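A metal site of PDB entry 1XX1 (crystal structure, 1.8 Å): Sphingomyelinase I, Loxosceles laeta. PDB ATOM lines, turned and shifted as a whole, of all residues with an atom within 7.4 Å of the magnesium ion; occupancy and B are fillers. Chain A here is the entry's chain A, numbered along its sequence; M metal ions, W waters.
The side-chain amino group (NZ) of Lys 93 sits close to the side-chain carboxylate (OD1) of Asp 34 (3.7 Å).
N of Asp 34 lies close to ND2 of Asn 15.
The backbone carbonyl oxygen of Asp 34 is in hydrogen-bond range of the backbone NH of Tyr 46 (2.7 Å).
OE1 of Glu 32 is in hydrogen-bond range of N of Met 13 (2.8 Å).
O of Glu 32 sits at hydrogen-bond distance from N of Val 14 (2.8 Å).
The backbone carbonyl oxygen (O) of Ala 33 is in hydrogen-bond range of the backbone NH (N) of Asp 91 (2.7 Å).
N of Val 35 sits at hydrogen-bond distance from O of Asp 91 (2.9 Å).
The backbone carbonyl oxygen (O) of Val 35 lies within hydrogen-bond range of the backbone NH (N) of Lys 93.
Water W1 lies within hydrogen-bond range of the side-chain carboxylate (OE1) of Glu 32, the side-chain carboxylate (OD2) of Asp 34 and a ring nitrogen (NE2) of His 12.
Water W3 is bound to the magnesium ion (1.9 Å).
The magnesium ion is bound by the side-chain carboxylate (OD1) of Asp 34 (1.9 Å).
The magnesium ion is bound by OE2 of Glu 32 (2.0 Å).
OD2 of Asp 91 binds the magnesium ion (2.0 Å).
Water W2 binds the magnesium ion (2.0 Å).
Water W1 binds the magnesium ion, 2.0 Å away.
The magnesium ion has six donor atoms within binding distance.
Merely in contact with the magnesium ion: Lys 93 (3.9 Å).
Within 4 Å of the magnesium ion: Glu 32, Asp 34, Asp 91 and Lys 93.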
ATOM      1  N   HIS A  12      19.712  -2.197  11.765  1.00  0.00           N
ATOM      2  CA  HIS A  12      18.973  -1.188  11.033  1.00  0.00           C
ATOM      3  C   HIS A  12      19.042  -1.452   9.544  1.00  0.00           C
ATOM      4  O   HIS A  12      20.104  -1.715   9.007  1.00  0.00           O
ATOM      5  CB  HIS A  12      19.574   0.176  11.347  1.00  0.00           C
ATOM      6  CG  HIS A  12      18.945   1.294  10.564  1.00  0.00           C
ATOM      7  ND1 HIS A  12      19.685   2.201   9.853  1.00  0.00           N
ATOM      8  CD2 HIS A  12      17.640   1.625  10.378  1.00  0.00           C
ATOM      9  CE1 HIS A  12      18.863   3.065   9.276  1.00  0.00           C
ATOM     10  NE2 HIS A  12      17.621   2.748   9.594  1.00  0.00           N
ATOM     11  N   MET A  13      17.888  -1.367   8.888  1.00  0.00           N
ATOM     12  CA  MET A  13      17.835  -1.329   7.435  1.00  0.00           C
ATOM     13  C   MET A  13      18.491  -2.546   6.821  1.00  0.00           C
ATOM     14  O   MET A  13      19.457  -2.451   6.084  1.00  0.00           O
ATOM     15  CB  MET A  13      18.514  -0.045   6.937  1.00  0.00           C
ATOM     16  CG  MET A  13      18.085   0.296   5.525  1.00  0.00           C
ATOM     17  SD  MET A  13      18.978   1.745   4.920  1.00  0.00           S
ATOM     18  CE  MET A  13      20.689   1.203   5.002  1.00  0.00           C
ATOM     19  N   VAL A  14      17.938  -3.707   7.152  1.00  0.00           N
ATOM     20  CA  VAL A  14      18.463  -4.965   6.629  1.00  0.00           C
ATOM     21  C   VAL A  14      17.495  -5.450   5.580  1.00  0.00           C
ATOM     22  O   VAL A  14      16.516  -6.158   5.899  1.00  0.00           O
ATOM     23  CB  VAL A  14      18.633  -5.999   7.757  1.00  0.00           C
ATOM     24  CG1 VAL A  14      19.351  -7.238   7.198  1.00  0.00           C
ATOM     25  CG2 VAL A  14      19.508  -5.380   8.851  1.00  0.00           C
ATOM     26  N   ASN A  15      17.730  -5.007   4.347  1.00  0.00           N
ATOM     27  CA  ASN A  15      16.744  -5.241   3.294  1.00  0.00           C
ATOM     28  C   ASN A  15      17.113  -6.288   2.258  1.00  0.00           C
ATOM     29  O   ASN A  15      16.292  -6.613   1.387  1.00  0.00           O
ATOM     30  CB  ASN A  15      16.414  -3.921   2.630  1.00  0.00           C
ATOM     31  CG  ASN A  15      15.720  -2.981   3.584  1.00  0.00           C
ATOM     32  OD1 ASN A  15      16.001  -1.770   3.647  1.00  0.00           O
ATOM     33  ND2 ASN A  15      14.798  -3.529   4.305  1.00  0.00           N
ATOM     34  N   GLU A  32      15.535  -4.859  11.303  1.00  0.00           N
ATOM     35  CA  GLU A  32      14.474  -3.990  10.840  1.00  0.00           C
ATOM     36  C   GLU A  32      14.608  -3.954   9.321  1.00  0.00           C
ATOM     37  O   GLU A  32      15.718  -3.869   8.805  1.00  0.00           O
ATOM     38  CB  GLU A  32      14.637  -2.587  11.411  1.00  0.00           C
ATOM     39  CG  GLU A  32      13.601  -1.675  10.909  1.00  0.00           C
ATOM     40  CD  GLU A  32      14.108  -0.730   9.844  1.00  0.00           C
ATOM     41  OE1 GLU A  32      15.331  -0.617   9.602  1.00  0.00           O
ATOM     42  OE2 GLU A  32      13.250  -0.009   9.286  1.00  0.00           O
ATOM     43  N   ALA A  33      13.479  -4.121   8.656  1.00  0.00           N
ATOM     44  CA  ALA A  33      13.426  -4.124   7.169  1.00  0.00           C
ATOM     45  C   ALA A  33      12.360  -3.138   6.763  1.00  0.00           C
ATOM     46  O   ALA A  33      11.346  -2.985   7.425  1.00  0.00           O
ATOM     47  CB  ALA A  33      13.114  -5.499   6.600  1.00  0.00           C
ATOM     48  N   ASP A  34      12.609  -2.472   5.639  1.00  0.00           N
ATOM     49  CA  ASP A  34      11.714  -1.443   5.150  1.00  0.00           C
ATOM     50  C   ASP A  34      10.882  -2.079   4.072  1.00  0.00           C
ATOM     51  O   ASP A  34      11.403  -2.465   3.056  1.00  0.00           O
ATOM     52  CB  ASP A  34      12.576  -0.370   4.501  1.00  0.00           C
ATOM     53  CG  ASP A  34      13.449   0.286   5.509  1.00  0.00           C
ATOM     54  OD1 ASP A  34      12.900   0.858   6.440  1.00  0.00           O
ATOM     55  OD2 ASP A  34      14.675   0.186   5.444  1.00  0.00           O
ATOM     56  N   VAL A  35       9.592  -2.147   4.316  1.00  0.00           N
ATOM     57  CA  VAL A  35       8.676  -2.851   3.432  1.00  0.00           C
ATOM     58  C   VAL A  35       8.021  -1.785   2.575  1.00  0.00           C
ATOM     59  O   VAL A  35       7.254  -0.948   3.095  1.00  0.00           O
ATOM     60  CB  VAL A  35       7.606  -3.583   4.241  1.00  0.00           C
ATOM     61  CG1 VAL A  35       6.585  -4.209   3.289  1.00  0.00           C
ATOM     62  CG2 VAL A  35       8.275  -4.669   5.134  1.00  0.00           C
ATOM     63  N   TYR A  46      13.275  -2.687   1.062  1.00  0.00           N
ATOM     64  CA  TYR A  46      14.077  -1.717   0.346  1.00  0.00           C
ATOM     65  C   TYR A  46      13.894  -0.350   0.996  1.00  0.00           C
ATOM     66  O   TYR A  46      12.768   0.051   1.272  1.00  0.00           O
ATOM     67  CB  TYR A  46      13.598  -1.616  -1.088  1.00  0.00           C
ATOM     68  CG  TYR A  46      14.220  -0.482  -1.876  1.00  0.00           C
ATOM     69  CD1 TYR A  46      15.544  -0.570  -2.321  1.00  0.00           C
ATOM     70  CD2 TYR A  46      13.480   0.665  -2.180  1.00  0.00           C
ATOM     71  CE1 TYR A  46      16.121   0.457  -3.087  1.00  0.00           C
ATOM     72  CE2 TYR A  46      14.054   1.710  -2.918  1.00  0.00           C
ATOM     73  CZ  TYR A  46      15.348   1.592  -3.380  1.00  0.00           C
ATOM     74  OH  TYR A  46      15.901   2.615  -4.139  1.00  0.00           O
ATOM     75  N   HIS A  47      14.993   0.330   1.193  1.00  0.00           N
ATOM     76  CA  HIS A  47      14.972   1.627   1.834  1.00  0.00           C
ATOM     77  C   HIS A  47      15.089   2.756   0.813  1.00  0.00           C
ATOM     78  O   HIS A  47      14.241   3.649   0.753  1.00  0.00           O
ATOM     79  CB  HIS A  47      16.136   1.728   2.789  1.00  0.00           C
ATOM     80  CG  HIS A  47      16.116   2.969   3.592  1.00  0.00           C
ATOM     81  ND1 HIS A  47      16.647   4.161   3.114  1.00  0.00           N
ATOM     82  CD2 HIS A  47      15.617   3.238   4.815  1.00  0.00           C
ATOM     83  CE1 HIS A  47      16.529   5.090   4.050  1.00  0.00           C
ATOM     84  NE2 HIS A  47      15.843   4.576   5.067  1.00  0.00           N
ATOM     85  N   VAL A  89      11.405  -5.973  12.901  1.00  0.00           N
ATOM     86  CA  VAL A  89      10.502  -4.858  12.742  1.00  0.00           C
ATOM     87  C   VAL A  89      10.285  -4.696  11.264  1.00  0.00           C
ATOM     88  O   VAL A  89      11.258  -4.590  10.499  1.00  0.00           O
ATOM     89  CB  VAL A  89      11.138  -3.579  13.265  1.00  0.00           C
ATOM     90  CG1 VAL A  89      10.338  -2.333  12.877  1.00  0.00           C
ATOM     91  CG2 VAL A  89      11.313  -3.670  14.783  1.00  0.00           C
ATOM     92  N   LEU A  90       9.018  -4.683  10.860  1.00  0.00           N
ATOM     93  CA  LEU A  90       8.674  -4.304   9.491  1.00  0.00           C
ATOM     94  C   LEU A  90       8.368  -2.850   9.529  1.00  0.00           C
ATOM     95  O   LEU A  90       7.367  -2.439  10.092  1.00  0.00           O
ATOM     96  CB  LEU A  90       7.482  -5.074   8.971  1.00  0.00           C
ATOM     97  CG  LEU A  90       7.778  -6.589   8.882  1.00  0.00           C
ATOM     98  CD1 LEU A  90       6.568  -7.351   8.287  1.00  0.00           C
ATOM     99  CD2 LEU A  90       9.027  -6.879   8.114  1.00  0.00           C
ATOM    100  N   ASP A  91       9.271  -2.080   8.950  1.00  0.00           N
ATOM    101  CA  ASP A  91       9.079  -0.636   8.826  1.00  0.00           C
ATOM    102  C   ASP A  91       8.214  -0.461   7.567  1.00  0.00           C
ATOM    103  O   ASP A  91       8.702  -0.453   6.455  1.00  0.00           O
ATOM    104  CB  ASP A  91      10.457   0.010   8.722  1.00  0.00           C
ATOM    105  CG  ASP A  91      10.408   1.510   8.677  1.00  0.00           C
ATOM    106  OD1 ASP A  91       9.309   2.085   8.722  1.00  0.00           O
ATOM    107  OD2 ASP A  91      11.526   2.098   8.578  1.00  0.00           O
ATOM    108  N   LEU A  92       6.913  -0.366   7.787  1.00  0.00           N
ATOM    109  CA  LEU A  92       5.974  -0.453   6.680  1.00  0.00           C
ATOM    110  C   LEU A  92       5.793   0.917   6.052  1.00  0.00           C
ATOM    111  O   LEU A  92       5.288   1.823   6.678  1.00  0.00           O
ATOM    112  CB  LEU A  92       4.625  -1.000   7.158  1.00  0.00           C
ATOM    113  CG  LEU A  92       4.788  -2.395   7.789  1.00  0.00           C
ATOM    114  CD1 LEU A  92       3.827  -2.598   8.960  1.00  0.00           C
ATOM    115  CD2 LEU A  92       4.625  -3.434   6.682  1.00  0.00           C
ATOM    116  N   LYS A  93       6.150   1.014   4.785  1.00  0.00           N
ATOM    117  CA  LYS A  93       6.223   2.304   4.114  1.00  0.00           C
ATOM    118  C   LYS A  93       4.893   2.592   3.444  1.00  0.00           C
ATOM    119  O   LYS A  93       4.800   2.605   2.213  1.00  0.00           O
ATOM    120  CB  LYS A  93       7.398   2.322   3.120  1.00  0.00           C
ATOM    121  CG  LYS A  93       8.722   2.006   3.857  1.00  0.00           C
ATOM    122  CD  LYS A  93       9.037   3.072   4.889  1.00  0.00           C
ATOM    123  CE  LYS A  93      10.493   2.929   5.345  1.00  0.00           C
ATOM    124  NZ  LYS A  93      10.794   3.904   6.417  1.00  0.00           N
ATOM    125  N   TRP A 230      16.449   5.011  17.599  1.00  0.00           N
ATOM    126  CA  TRP A 230      17.095   4.620  16.387  1.00  0.00           C
ATOM    127  C   TRP A 230      18.195   5.453  15.823  1.00  0.00           C
ATOM    128  O   TRP A 230      18.280   6.641  16.088  1.00  0.00           O
ATOM    129  CB  TRP A 230      16.175   3.919  15.388  1.00  0.00           C
ATOM    130  CG  TRP A 230      15.644   4.602  14.206  1.00  0.00           C
ATOM    131  CD1 TRP A 230      16.341   5.110  13.132  1.00  0.00           C
ATOM    132  CD2 TRP A 230      14.269   4.716  13.882  1.00  0.00           C
ATOM    133  NE1 TRP A 230      15.458   5.606  12.190  1.00  0.00           N
ATOM    134  CE2 TRP A 230      14.176   5.373  12.623  1.00  0.00           C
ATOM    135  CE3 TRP A 230      13.076   4.367  14.547  1.00  0.00           C
ATOM    136  CZ2 TRP A 230      12.947   5.671  12.029  1.00  0.00           C
ATOM    137  CZ3 TRP A 230      11.845   4.679  13.950  1.00  0.00           C
ATOM    138  CH2 TRP A 230      11.804   5.327  12.704  1.00  0.00           C
ATOM    139  N   MET A 250      18.256   0.577  17.763  1.00  0.00           N
ATOM    140  CA  MET A 250      18.332   0.328  16.366  1.00  0.00           C
ATOM    141  C   MET A 250      19.658   0.876  15.924  1.00  0.00           C
ATOM    142  O   MET A 250      19.973   2.021  16.186  1.00  0.00           O
ATOM    143  CB  MET A 250      17.254   1.026  15.614  1.00  0.00           C
ATOM    144  CG  MET A 250      17.525   0.990  14.160  1.00  0.00           C
ATOM    145  SD  MET A 250      16.416  -0.232  13.577  1.00  0.00           S
ATOM    146  CE  MET A 250      15.182   0.881  13.122  1.00  0.00           C
HETATM  147 MG    MG M   1      13.388   1.592   8.176  1.00  0.00          MG
HETATM  148  O   HOH W   1      15.345   1.176   7.810  1.00  0.00           O
HETATM  149  O   HOH W   2      13.841   2.666   9.797  1.00  0.00           O
HETATM  150  O   HOH W   3      13.403   3.289   7.285  1.00  0.00           O
